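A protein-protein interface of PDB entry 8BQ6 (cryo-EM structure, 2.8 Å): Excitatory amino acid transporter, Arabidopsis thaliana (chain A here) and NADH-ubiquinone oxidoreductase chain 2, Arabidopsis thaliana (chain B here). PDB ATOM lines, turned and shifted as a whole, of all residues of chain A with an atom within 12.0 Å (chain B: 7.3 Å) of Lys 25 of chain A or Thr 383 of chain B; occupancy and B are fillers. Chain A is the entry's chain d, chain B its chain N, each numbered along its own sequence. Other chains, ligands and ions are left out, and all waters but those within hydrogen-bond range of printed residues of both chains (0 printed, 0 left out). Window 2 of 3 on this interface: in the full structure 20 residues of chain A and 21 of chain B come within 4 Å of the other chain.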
ATOM      1  N   THR A  16     -14.834 -15.252 -16.570  1.00  0.00           N
ATOM      2  CA  THR A  16     -15.808 -15.356 -15.490  1.00  0.00           C
ATOM      3  C   THR A  16     -15.608 -16.644 -14.707  1.00  0.00           C
ATOM      4  O   THR A  16     -15.628 -16.641 -13.472  1.00  0.00           O
ATOM      5  CB  THR A  16     -17.232 -15.274 -16.039  1.00  0.00           C
ATOM      6  OG1 THR A  16     -17.415 -14.026 -16.714  1.00  0.00           O
ATOM      7  CG2 THR A  16     -18.231 -15.349 -14.907  1.00  0.00           C
ATOM      8  N   GLN A  17     -15.308 -17.754 -15.380  1.00  0.00           N
ATOM      9  CA  GLN A  17     -15.093 -19.047 -14.669  1.00  0.00           C
ATOM     10  C   GLN A  17     -13.805 -18.979 -13.835  1.00  0.00           C
ATOM     11  O   GLN A  17     -13.844 -19.399 -12.667  1.00  0.00           O
ATOM     12  CB  GLN A  17     -15.134 -20.232 -15.640  1.00  0.00           C
ATOM     13  CG  GLN A  17     -14.979 -21.595 -14.977  1.00  0.00           C
ATOM     14  CD  GLN A  17     -15.892 -21.854 -13.803  1.00  0.00           C
ATOM     15  OE1 GLN A  17     -17.111 -21.728 -13.889  1.00  0.00           O
ATOM     16  NE2 GLN A  17     -15.300 -22.248 -12.689  1.00  0.00           N
ATOM     17  N   MET A  18     -12.731 -18.408 -14.382  1.00  0.00           N
ATOM     18  CA  MET A  18     -11.448 -18.262 -13.640  1.00  0.00           C
ATOM     19  C   MET A  18     -11.626 -17.330 -12.439  1.00  0.00           C
ATOM     20  O   MET A  18     -11.145 -17.699 -11.361  1.00  0.00           O
ATOM     21  CB  MET A  18     -10.367 -17.708 -14.569  1.00  0.00           C
ATOM     22  CG  MET A  18      -9.870 -18.741 -15.556  1.00  0.00           C
ATOM     23  SD  MET A  18      -8.357 -18.230 -16.391  1.00  0.00           S
ATOM     24  CE  MET A  18      -9.026 -17.060 -17.571  1.00  0.00           C
ATOM     25  N   TYR A  19     -12.266 -16.174 -12.619  1.00  0.00           N
ATOM     26  CA  TYR A  19     -12.559 -15.213 -11.525  1.00  0.00           C
ATOM     27  C   TYR A  19     -13.320 -15.926 -10.400  1.00  0.00           C
ATOM     28  O   TYR A  19     -12.911 -15.800  -9.248  1.00  0.00           O
ATOM     29  CB  TYR A  19     -13.397 -14.081 -12.120  1.00  0.00           C
ATOM     30  CG  TYR A  19     -13.342 -12.721 -11.478  1.00  0.00           C
ATOM     31  CD1 TYR A  19     -12.820 -12.523 -10.213  1.00  0.00           C
ATOM     32  CD2 TYR A  19     -13.845 -11.623 -12.153  1.00  0.00           C
ATOM     33  CE1 TYR A  19     -12.792 -11.265  -9.638  1.00  0.00           C
ATOM     34  CE2 TYR A  19     -13.824 -10.357 -11.595  1.00  0.00           C
ATOM     35  CZ  TYR A  19     -13.295 -10.180 -10.332  1.00  0.00           C
ATOM     36  OH  TYR A  19     -13.265  -8.935  -9.780  1.00  0.00           O
ATOM     37  N   SER A  20     -14.400 -16.626 -10.736  1.00  0.00           N
ATOM     38  CA  SER A  20     -15.180 -17.411  -9.746  1.00  0.00           C
ATOM     39  C   SER A  20     -14.258 -18.355  -8.964  1.00  0.00           C
ATOM     40  O   SER A  20     -14.283 -18.288  -7.723  1.00  0.00           O
ATOM     41  CB  SER A  20     -16.298 -18.144 -10.436  1.00  0.00           C
ATOM     42  OG  SER A  20     -16.790 -19.214  -9.646  1.00  0.00           O
ATOM     43  N   ASN A  21     -13.468 -19.179  -9.655  1.00  0.00           N
ATOM     44  CA  ASN A  21     -12.527 -20.127  -8.996  1.00  0.00           C
ATOM     45  C   ASN A  21     -11.573 -19.374  -8.060  1.00  0.00           C
ATOM     46  O   ASN A  21     -11.378 -19.846  -6.940  1.00  0.00           O
ATOM     47  CB  ASN A  21     -11.755 -20.966 -10.018  1.00  0.00           C
ATOM     48  CG  ASN A  21     -12.485 -22.206 -10.480  1.00  0.00           C
ATOM     49  OD1 ASN A  21     -13.404 -22.683  -9.819  1.00  0.00           O
ATOM     50  ND2 ASN A  21     -12.078 -22.737 -11.618  1.00  0.00           N
ATOM     51  N   ALA A  22     -11.037 -18.232  -8.494  1.00  0.00           N
ATOM     52  CA  ALA A  22     -10.083 -17.441  -7.684  1.00  0.00           C
ATOM     53  C   ALA A  22     -10.762 -16.856  -6.443  1.00  0.00           C
ATOM     54  O   ALA A  22     -10.129 -16.887  -5.381  1.00  0.00           O
ATOM     55  CB  ALA A  22      -9.477 -16.356  -8.534  1.00  0.00           C
ATOM     56  N   LEU A  23     -11.986 -16.334  -6.572  1.00  0.00           N
ATOM     57  CA  LEU A  23     -12.731 -15.754  -5.419  1.00  0.00           C
ATOM     58  C   LEU A  23     -12.998 -16.845  -4.379  1.00  0.00           C
ATOM     59  O   LEU A  23     -13.165 -16.490  -3.205  1.00  0.00           O
ATOM     60  CB  LEU A  23     -14.043 -15.138  -5.910  1.00  0.00           C
ATOM     61  CG  LEU A  23     -13.939 -13.768  -6.577  1.00  0.00           C
ATOM     62  CD1 LEU A  23     -15.222 -13.439  -7.319  1.00  0.00           C
ATOM     63  CD2 LEU A  23     -13.621 -12.687  -5.558  1.00  0.00           C
ATOM     64  N   ARG A  24     -13.024 -18.112  -4.795  1.00  0.00           N
ATOM     65  CA  ARG A  24     -13.254 -19.259  -3.882  1.00  0.00           C
ATOM     66  C   ARG A  24     -11.926 -19.918  -3.483  1.00  0.00           C
ATOM     67  O   ARG A  24     -11.990 -21.051  -2.981  1.00  0.00           O
ATOM     68  CB  ARG A  24     -14.123 -20.279  -4.611  1.00  0.00           C
ATOM     69  CG  ARG A  24     -15.545 -19.821  -4.881  1.00  0.00           C
ATOM     70  CD  ARG A  24     -16.152 -20.729  -5.923  1.00  0.00           C
ATOM     71  NE  ARG A  24     -16.648 -21.957  -5.329  1.00  0.00           N
ATOM     72  CZ  ARG A  24     -16.818 -23.094  -5.987  1.00  0.00           C
ATOM     73  NH1 ARG A  24     -16.529 -23.167  -7.275  1.00  0.00           N
ATOM     74  NH2 ARG A  24     -17.277 -24.154  -5.351  1.00  0.00           N
ATOM     75  N   LYS A  25     -10.782 -19.256  -3.704  1.00  0.00           N
ATOM     76  CA  LYS A  25      -9.421 -19.788  -3.370  1.00  0.00           C
ATOM     77  C   LYS A  25      -9.178 -21.165  -4.010  1.00  0.00           C
ATOM     78  O   LYS A  25      -8.411 -21.947  -3.435  1.00  0.00           O
ATOM     79  CB  LYS A  25      -9.186 -19.803  -1.854  1.00  0.00           C
ATOM     80  CG  LYS A  25      -9.668 -18.568  -1.107  1.00  0.00           C
ATOM     81  CD  LYS A  25      -8.825 -18.245   0.094  1.00  0.00           C
ATOM     82  CE  LYS A  25      -7.640 -17.372  -0.252  1.00  0.00           C
ATOM     83  NZ  LYS A  25      -6.595 -17.447   0.796  1.00  0.00           N
ATOM     84  N   LEU A  26      -9.789 -21.436  -5.159  1.00  0.00           N
ATOM     85  CA  LEU A  26      -9.569 -22.710  -5.885  1.00  0.00           C
ATOM     86  C   LEU A  26      -8.539 -22.467  -6.984  1.00  0.00           C
ATOM     87  O   LEU A  26      -8.346 -21.290  -7.360  1.00  0.00           O
ATOM     88  CB  LEU A  26     -10.901 -23.169  -6.481  1.00  0.00           C
ATOM     89  CG  LEU A  26     -11.939 -23.664  -5.479  1.00  0.00           C
ATOM     90  CD1 LEU A  26     -13.171 -24.179  -6.203  1.00  0.00           C
ATOM     91  CD2 LEU A  26     -11.357 -24.746  -4.585  1.00  0.00           C
ATOM     92  N   PRO A  27      -7.843 -23.497  -7.509  1.00  0.00           N
ATOM     93  CA  PRO A  27      -6.951 -23.292  -8.660  1.00  0.00           C
ATOM     94  C   PRO A  27      -7.732 -22.685  -9.835  1.00  0.00           C
ATOM     95  O   PRO A  27      -8.876 -23.035 -10.023  1.00  0.00           O
ATOM     96  CB  PRO A  27      -6.482 -24.706  -9.001  1.00  0.00           C
ATOM     97  CG  PRO A  27      -6.585 -25.448  -7.689  1.00  0.00           C
ATOM     98  CD  PRO A  27      -7.805 -24.870  -7.007  1.00  0.00           C
ATOM     99  N   TYR A  28      -7.088 -21.819 -10.620  1.00  0.00           N
ATOM    100  CA  TYR A  28      -7.768 -21.144 -11.756  1.00  0.00           C
ATOM    101  C   TYR A  28      -8.454 -22.155 -12.666  1.00  0.00           C
ATOM    102  O   TYR A  28      -9.559 -21.846 -13.099  1.00  0.00           O
ATOM    103  CB  TYR A  28      -6.773 -20.361 -12.612  1.00  0.00           C
ATOM    104  CG  TYR A  28      -6.518 -18.940 -12.186  1.00  0.00           C
ATOM    105  CD1 TYR A  28      -5.225 -18.459 -12.069  1.00  0.00           C
ATOM    106  CD2 TYR A  28      -7.561 -18.070 -11.925  1.00  0.00           C
ATOM    107  CE1 TYR A  28      -4.972 -17.151 -11.689  1.00  0.00           C
ATOM    108  CE2 TYR A  28      -7.326 -16.758 -11.551  1.00  0.00           C
ATOM    109  CZ  TYR A  28      -6.028 -16.299 -11.429  1.00  0.00           C
ATOM    110  OH  TYR A  28      -5.784 -15.010 -11.054  1.00  0.00           O
ATOM    111  N   MET A  29      -7.838 -23.314 -12.915  1.00  0.00           N
ATOM    112  CA  MET A  29      -8.392 -24.275 -13.902  1.00  0.00           C
ATOM    113  C   MET A  29      -9.104 -25.453 -13.229  1.00  0.00           C
ATOM    114  O   MET A  29      -9.248 -26.496 -13.890  1.00  0.00           O
ATOM    115  CB  MET A  29      -7.277 -24.783 -14.820  1.00  0.00           C
ATOM    116  CG  MET A  29      -6.745 -23.717 -15.750  1.00  0.00           C
ATOM    117  SD  MET A  29      -7.986 -23.115 -16.917  1.00  0.00           S
ATOM    118  CE  MET A  29      -8.547 -24.651 -17.649  1.00  0.00           C
ATOM    119  N   ARG A  30      -9.570 -25.290 -11.993  1.00  0.00           N
ATOM    120  CA  ARG A  30     -10.379 -26.350 -11.336  1.00  0.00           C
ATOM    121  C   ARG A  30     -11.672 -26.548 -12.142  1.00  0.00           C
ATOM    122  O   ARG A  30     -12.334 -25.536 -12.415  1.00  0.00           O
ATOM    123  CB  ARG A  30     -10.627 -25.956  -9.877  1.00  0.00           C
ATOM    124  CG  ARG A  30     -11.573 -26.868  -9.113  1.00  0.00           C
ATOM    125  CD  ARG A  30     -10.996 -28.240  -8.826  1.00  0.00           C
ATOM    126  NE  ARG A  30      -9.696 -28.245  -8.170  1.00  0.00           N
ATOM    127  CZ  ARG A  30      -9.508 -28.296  -6.856  1.00  0.00           C
ATOM    128  NH1 ARG A  30     -10.543 -28.334  -6.033  1.00  0.00           N
ATOM    129  NH2 ARG A  30      -8.283 -28.309  -6.366  1.00  0.00           N
ATOM    130  N   HIS A  31     -12.004 -27.792 -12.512  1.00  0.00           N
ATOM    131  CA  HIS A  31     -13.202 -28.114 -13.347  1.00  0.00           C
ATOM    132  C   HIS A  31     -13.136 -27.415 -14.724  1.00  0.00           C
ATOM    133  O   HIS A  31     -13.979 -26.555 -14.977  1.00  0.00           O
ATOM    134  CB  HIS A  31     -14.496 -27.868 -12.554  1.00  0.00           C
ATOM    135  CG  HIS A  31     -14.645 -28.685 -11.316  1.00  0.00           C
ATOM    136  ND1 HIS A  31     -15.761 -28.595 -10.513  1.00  0.00           N
ATOM    137  CD2 HIS A  31     -13.844 -29.607 -10.741  1.00  0.00           C
ATOM    138  CE1 HIS A  31     -15.639 -29.422  -9.497  1.00  0.00           C
ATOM    139  NE2 HIS A  31     -14.471 -30.052  -9.612  1.00  0.00           N
ATOM    140  N   HIS A  35     -15.034 -24.295 -17.696  1.00  0.00           N
ATOM    141  CA  HIS A  35     -14.406 -23.203 -18.485  1.00  0.00           C
ATOM    142  C   HIS A  35     -14.936 -23.274 -19.917  1.00  0.00           C
ATOM    143  O   HIS A  35     -15.179 -22.210 -20.497  1.00  0.00           O
ATOM    144  CB  HIS A  35     -12.878 -23.277 -18.412  1.00  0.00           C
ATOM    145  CG  HIS A  35     -12.326 -23.049 -17.049  1.00  0.00           C
ATOM    146  ND1 HIS A  35     -12.438 -23.980 -16.042  1.00  0.00           N
ATOM    147  CD2 HIS A  35     -11.663 -22.001 -16.523  1.00  0.00           C
ATOM    148  CE1 HIS A  35     -11.868 -23.519 -14.955  1.00  0.00           C
ATOM    149  NE2 HIS A  35     -11.392 -22.306 -15.224  1.00  0.00           N
ATOM    150  N   LEU B 377     -12.221  -5.807   8.292  1.00  0.00           N
ATOM    151  CA  LEU B 377     -11.665  -6.033   6.936  1.00  0.00           C
ATOM    152  C   LEU B 377     -10.144  -5.784   6.917  1.00  0.00           C
ATOM    153  O   LEU B 377      -9.588  -5.765   5.813  1.00  0.00           O
ATOM    154  CB  LEU B 377     -12.388  -5.114   5.949  1.00  0.00           C
ATOM    155  CG  LEU B 377     -13.912  -5.168   5.977  1.00  0.00           C
ATOM    156  CD1 LEU B 377     -14.500  -3.935   5.311  1.00  0.00           C
ATOM    157  CD2 LEU B 377     -14.407  -6.428   5.297  1.00  0.00           C
ATOM    158  N   GLY B 378      -9.495  -5.636   8.078  1.00  0.00           N
ATOM    159  CA  GLY B 378      -8.062  -5.397   8.081  1.00  0.00           C
ATOM    160  C   GLY B 378      -7.292  -6.585   7.533  1.00  0.00           C
ATOM    161  O   GLY B 378      -7.587  -7.741   7.843  1.00  0.00           O
ATOM    162  N   ALA B 379      -6.289  -6.284   6.709  1.00  0.00           N
ATOM    163  CA  ALA B 379      -5.420  -7.270   6.068  1.00  0.00           C
ATOM    164  C   ALA B 379      -6.182  -8.246   5.181  1.00  0.00           C
ATOM    165  O   ALA B 379      -5.769  -9.399   5.033  1.00  0.00           O
ATOM    166  CB  ALA B 379      -4.592  -8.044   7.101  1.00  0.00           C
ATOM    167  N   LEU B 380      -7.287  -7.819   4.567  1.00  0.00           N
ATOM    168  CA  LEU B 380      -7.989  -8.715   3.656  1.00  0.00           C
ATOM    169  C   LEU B 380      -7.257  -8.838   2.326  1.00  0.00           C
ATOM    170  O   LEU B 380      -7.452  -9.815   1.595  1.00  0.00           O
ATOM    171  CB  LEU B 380      -9.425  -8.235   3.442  1.00  0.00           C
ATOM    172  CG  LEU B 380     -10.344  -9.097   2.572  1.00  0.00           C
ATOM    173  CD1 LEU B 380     -10.613 -10.442   3.230  1.00  0.00           C
ATOM    174  CD2 LEU B 380     -11.641  -8.370   2.296  1.00  0.00           C
ATOM    175  N   ALA B 381      -6.398  -7.872   2.002  1.00  0.00           N
ATOM    176  CA  ALA B 381      -5.634  -7.963   0.766  1.00  0.00           C
ATOM    177  C   ALA B 381      -4.518  -8.994   0.859  1.00  0.00           C
ATOM    178  O   ALA B 381      -3.983  -9.407  -0.175  1.00  0.00           O
ATOM    179  CB  ALA B 381      -5.072  -6.592   0.401  1.00  0.00           C
ATOM    180  N   LYS B 382      -4.156  -9.418   2.068  1.00  0.00           N
ATOM    181  CA  LYS B 382      -3.229 -10.527   2.244  1.00  0.00           C
ATOM    182  C   LYS B 382      -3.947 -11.867   2.287  1.00  0.00           C
ATOM    183  O   LYS B 382      -3.541 -12.813   1.606  1.00  0.00           O
ATOM    184  CB  LYS B 382      -2.424 -10.352   3.531  1.00  0.00           C
ATOM    185  CG  LYS B 382      -1.638  -9.075   3.596  1.00  0.00           C
ATOM    186  CD  LYS B 382      -0.225  -9.308   3.144  1.00  0.00           C
ATOM    187  CE  LYS B 382       0.145  -8.341   2.041  1.00  0.00           C
ATOM    188  NZ  LYS B 382       1.248  -8.862   1.191  1.00  0.00           N
ATOM    189  N   THR B 383      -5.010 -11.961   3.084  1.00  0.00           N
ATOM    190  CA  THR B 383      -5.714 -13.221   3.262  1.00  0.00           C
ATOM    191  C   THR B 383      -6.548 -13.618   2.049  1.00  0.00           C
ATOM    192  O   THR B 383      -6.723 -14.815   1.806  1.00  0.00           O
ATOM    193  CB  THR B 383      -6.586 -13.151   4.520  1.00  0.00           C
ATOM    194  OG1 THR B 383      -7.622 -12.179   4.339  1.00  0.00           O
ATOM    195  CG2 THR B 383      -5.745 -12.775   5.724  1.00  0.00           C
ATOM    196  N   ASN B 384      -7.042 -12.657   1.276  1.00  0.00           N
ATOM    197  CA  ASN B 384      -7.817 -12.962   0.077  1.00  0.00           C
ATOM    198  C   ASN B 384      -7.666 -11.811  -0.908  1.00  0.00           C
ATOM    199  O   ASN B 384      -8.579 -10.987  -1.048  1.00  0.00           O
ATOM    200  CB  ASN B 384      -9.288 -13.197   0.431  1.00  0.00           C
ATOM    201  CG  ASN B 384     -10.046 -13.952  -0.650  1.00  0.00           C
ATOM    202  OD1 ASN B 384      -9.616 -14.018  -1.801  1.00  0.00           O
ATOM    203  ND2 ASN B 384     -11.186 -14.521  -0.281  1.00  0.00           N
ATOM    204  N   PRO B 385      -6.527 -11.721  -1.601  1.00  0.00           N
ATOM    205  CA  PRO B 385      -6.274 -10.534  -2.443  1.00  0.00           C
ATOM    206  C   PRO B 385      -7.310 -10.289  -3.531  1.00  0.00           C
ATOM    207  O   PRO B 385      -7.665  -9.130  -3.775  1.00  0.00           O
ATOM    208  CB  PRO B 385      -4.876 -10.810  -3.021  1.00  0.00           C
ATOM    209  CG  PRO B 385      -4.315 -11.937  -2.215  1.00  0.00           C
ATOM    210  CD  PRO B 385      -5.458 -12.724  -1.701  1.00  0.00           C
ATOM    211  N   ILE B 386      -7.821 -11.333  -4.188  1.00  0.00           N
ATOM    212  CA  ILE B 386      -8.769 -11.079  -5.271  1.00  0.00           C
ATOM    213  C   ILE B 386     -10.099 -10.570  -4.722  1.00  0.00           C
ATOM    214  O   ILE B 386     -10.766  -9.746  -5.362  1.00  0.00           O
ATOM    215  CB  ILE B 386      -8.949 -12.326  -6.160  1.00  0.00           C
ATOM    216  CG1 ILE B 386      -9.890 -12.009  -7.320  1.00  0.00           C
ATOM    217  CG2 ILE B 386      -9.486 -13.496  -5.370  1.00  0.00           C
ATOM    218  CD1 ILE B 386      -9.421 -10.843  -8.165  1.00  0.00           C
ATOM    219  N   LEU B 387     -10.500 -11.006  -3.524  1.00  0.00           N
ATOM    220  CA  LEU B 387     -11.739 -10.453  -2.911  1.00  0.00           C
ATOM    221  C   LEU B 387     -11.536  -8.971  -2.546  1.00  0.00           C
ATOM    222  O   LEU B 387     -12.454  -8.183  -2.807  1.00  0.00           O
ATOM    223  CB  LEU B 387     -12.131 -11.295  -1.695  1.00  0.00           C
ATOM    224  CG  LEU B 387     -13.397 -10.862  -0.957  1.00  0.00           C
ATOM    225  CD1 LEU B 387     -14.591 -10.816  -1.896  1.00  0.00           C
ATOM    226  CD2 LEU B 387     -13.675 -11.784   0.215  1.00  0.00           C
ATOM    227  N   MET B 447      -8.449  -2.341   4.012  1.00  0.00           N
ATOM    228  CA  MET B 447      -8.112  -3.674   3.460  1.00  0.00           C
ATOM    229  C   MET B 447      -6.679  -3.714   2.932  1.00  0.00           C
ATOM    230  O   MET B 447      -6.120  -4.810   2.900  1.00  0.00           O
ATOM    231  CB  MET B 447      -9.039  -4.034   2.296  1.00  0.00           C
ATOM    232  CG  MET B 447     -10.477  -4.257   2.694  1.00  0.00           C
ATOM    233  SD  MET B 447     -11.460  -4.749   1.263  1.00  0.00           S
ATOM    234  CE  MET B 447     -11.701  -3.166   0.460  1.00  0.00           C
ATOM    235  N   TRP B 455      -5.686 -10.590  12.996  1.00  0.00           N
ATOM    236  CA  TRP B 455      -6.373 -10.745  11.721  1.00  0.00           C
ATOM    237  C   TRP B 455      -7.589 -11.648  11.886  1.00  0.00           C
ATOM    238  O   TRP B 455      -7.616 -12.534  12.742  1.00  0.00           O
ATOM    239  CB  TRP B 455      -5.450 -11.346  10.652  1.00  0.00           C
ATOM    240  CG  TRP B 455      -4.232 -10.538  10.293  1.00  0.00           C
ATOM    241  CD1 TRP B 455      -3.771  -9.423  10.921  1.00  0.00           C
ATOM    242  CD2 TRP B 455      -3.317 -10.799   9.219  1.00  0.00           C
ATOM    243  NE1 TRP B 455      -2.629  -8.970  10.307  1.00  0.00           N
ATOM    244  CE2 TRP B 455      -2.330  -9.797   9.259  1.00  0.00           C
ATOM    245  CE3 TRP B 455      -3.238 -11.783   8.230  1.00  0.00           C
ATOM    246  CZ2 TRP B 455      -1.278  -9.749   8.348  1.00  0.00           C
ATOM    247  CZ3 TRP B 455      -2.195 -11.732   7.325  1.00  0.00           C
ATOM    248  CH2 TRP B 455      -1.230 -10.722   7.390  1.00  0.00           C
ATOM    249  N   ILE B 456      -8.597 -11.420  11.049  1.00  0.00           N
ATOM    250  CA  ILE B 456      -9.739 -12.318  10.932  1.00  0.00           C
ATOM    251  C   ILE B 456      -9.613 -13.046   9.605  1.00  0.00           C
ATOM    252  O   ILE B 456      -9.541 -12.413   8.546  1.00  0.00           O
ATOM    253  CB  ILE B 456     -11.075 -11.567  11.025  1.00  0.00           C
ATOM    254  CG1 ILE B 456     -11.352 -11.160  12.471  1.00  0.00           C
ATOM    255  CG2 ILE B 456     -12.212 -12.418  10.476  1.00  0.00           C
ATOM    256  CD1 ILE B 456     -12.249  -9.970  12.595  1.00  0.00           C
ATOM    257  N   LEU B 457      -9.573 -14.372   9.657  1.00  0.00           N
ATOM    258  CA  LEU B 457      -9.526 -15.180   8.448  1.00  0.00           C
ATOM    259  C   LEU B 457     -10.950 -15.563   8.069  1.00  0.00           C
ATOM    260  O   LEU B 457     -11.715 -16.051   8.908  1.00  0.00           O
ATOM    261  CB  LEU B 457      -8.645 -16.413   8.642  1.00  0.00           C
ATOM    262  CG  LEU B 457      -7.259 -16.135   9.231  1.00  0.00           C
ATOM    263  CD1 LEU B 457      -6.419 -17.400   9.287  1.00  0.00           C
ATOM    264  CD2 LEU B 457      -6.549 -15.064   8.433  1.00  0.00           C
ATOM    265  N   TYR B 458     -11.306 -15.321   6.814  1.00  0.00           N
ATOM    266  CA  TYR B 458     -12.670 -15.488   6.343  1.00  0.00           C
ATOM    267  C   TYR B 458     -12.788 -16.761   5.522  1.00  0.00           C
ATOM    268  O   TYR B 458     -11.869 -17.126   4.785  1.00  0.00           O
ATOM    269  CB  TYR B 458     -13.109 -14.285   5.506  1.00  0.00           C
ATOM    270  CG  TYR B 458     -13.242 -13.017   6.310  1.00  0.00           C
ATOM    271  CD1 TYR B 458     -14.416 -12.729   6.984  1.00  0.00           C
ATOM    272  CD2 TYR B 458     -12.199 -12.100   6.386  1.00  0.00           C
ATOM    273  CE1 TYR B 458     -14.548 -11.583   7.722  1.00  0.00           C
ATOM    274  CE2 TYR B 458     -12.325 -10.941   7.122  1.00  0.00           C
ATOM    275  CZ  TYR B 458     -13.505 -10.690   7.787  1.00  0.00           C
ATOM    276  OH  TYR B 458     -13.657  -9.543   8.527  1.00  0.00           O
ATOM    277  N   GLU B 459     -13.918 -17.441   5.672  1.00  0.00           N
ATOM    278  CA  GLU B 459     -14.192 -18.623   4.874  1.00  0.00           C
ATOM    279  C   GLU B 459     -14.450 -18.225   3.423  1.00  0.00           C
ATOM    280  O   GLU B 459     -15.074 -17.192   3.166  1.00  0.00           O
ATOM    281  CB  GLU B 459     -15.406 -19.362   5.426  1.00  0.00           C
ATOM    282  CG  GLU B 459     -15.238 -19.887   6.836  1.00  0.00           C
ATOM    283  CD  GLU B 459     -14.007 -20.749   6.989  1.00  0.00           C
ATOM    284  OE1 GLU B 459     -13.098 -20.353   7.746  1.00  0.00           O
ATOM    285  OE2 GLU B 459     -13.946 -21.818   6.349  1.00  0.00           O
ATOM    286  N   PRO B 460     -13.998 -19.022   2.456  1.00  0.00           N
ATOM    287  CA  PRO B 460     -14.277 -18.705   1.051  1.00  0.00           C
ATOM    288  C   PRO B 460     -15.764 -18.798   0.743  1.00  0.00           C
ATOM    289  O   PRO B 460     -16.503 -19.571   1.357  1.00  0.00           O
ATOM    290  CB  PRO B 460     -13.484 -19.765   0.281  1.00  0.00           C
ATOM    291  CG  PRO B 460     -13.308 -20.877   1.248  1.00  0.00           C
ATOM    292  CD  PRO B 460     -13.212 -20.259   2.602  1.00  0.00           C
ATOM    293  N   MET B 461     -16.200 -18.005  -0.230  1.00  0.00           N
ATOM    294  CA  MET B 461     -17.612 -17.949  -0.569  1.00  0.00           C
ATOM    295  C   MET B 461     -18.022 -19.143  -1.429  1.00  0.00           C
ATOM    296  O   MET B 461     -17.189 -19.857  -1.993  1.00  0.00           O
ATOM    297  CB  MET B 461     -17.934 -16.647  -1.291  1.00  0.00           C
ATOM    298  CG  MET B 461     -17.196 -16.466  -2.592  1.00  0.00           C
ATOM    299  SD  MET B 461     -17.772 -14.989  -3.422  1.00  0.00           S
ATOM    300  CE  MET B 461     -16.425 -13.894  -3.004  1.00  0.00           C
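Of the 17 printed residues of chain A, 5 touch a printed residue of chain B.
Hydrophobic or aromatic side chains of chain B that line the printed part of chain A: Ile 386, Pro 460 and Met 461.
Among the printed residues, 8 pairs touch across the chains.
Among the printed residues, no Asp or Glu carboxylate lies within 4 Å of a Lys or Arg side-chain nitrogen of the other chain.
Among the printed residues, merely in contact across the chains: Arg 24 of chain A with Met 461 of chain B (3.3 Å), Ala 22 of chain A with Ile 386 of chain B (3.5 Å), Tyr 19 of chain A with Ile 386 of chain B (3.7 Å), Arg 24 of chain A with Pro 460 of chain B (3.8 Å), Leu 23 of chain A with Leu 387 of chain B (3.9 Å), Leu 23 of chain A with Ile 386 of chain B (3.95 Å) and Leu 23 of chain A with Met 461 of chain B (3.96 Å).
O of Thr 383 of chain B is in hydrogen-bond range of NZ of Lys 25 of chain A, 2.8 Å away.
The backbone carbonyl oxygen (O) of Ala 379 of chain B lies within hydrogen-bond range of the side-chain hydroxyl (OG1) of Thr 383 of chain B (3.4 Å).
Lys 25 of chain A touches one residue of chain B.
No residue of chain A comes within 4 Å of Gly 378 of chain B.
No residue of chain A comes within 4 Å of Leu 380 of chain B.
No residue of chain A comes within 4 Å of Ala 381 of chain B.
No residue of chain A comes within 4 Å of Lys 382 of chain B.
No residue of chain A comes within 4 Å of Pro 385 of chain B.
No residue of chain A comes within 4 Å of Trp 455 of chain B.
No residue of chain A comes within 4 Å of Leu 457 of chain B.
No residue of chain A comes within 4 Å of Tyr 458 of chain B.
Of the printed residues of chain A, Leu 387 of chain B touches Leu 23 (3.9 Å).
Printed residues of chain A within 4 Å of Ile 386 of chain B: Tyr 19 (3.7 Å), Ala 22 (3.5 Å) and Leu 23 (3.95 Å).
Pro 27 of chain A touches none of the printed residues of chain B.
The nearest residue of chain A that does not touch Thr 383 of chain B is Ala 22 of chain A (8.2 Å).
The nearest printed residue of chain B that does not touch Tyr 19 of chain A is Leu 387 of chain B (6.5 Å).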
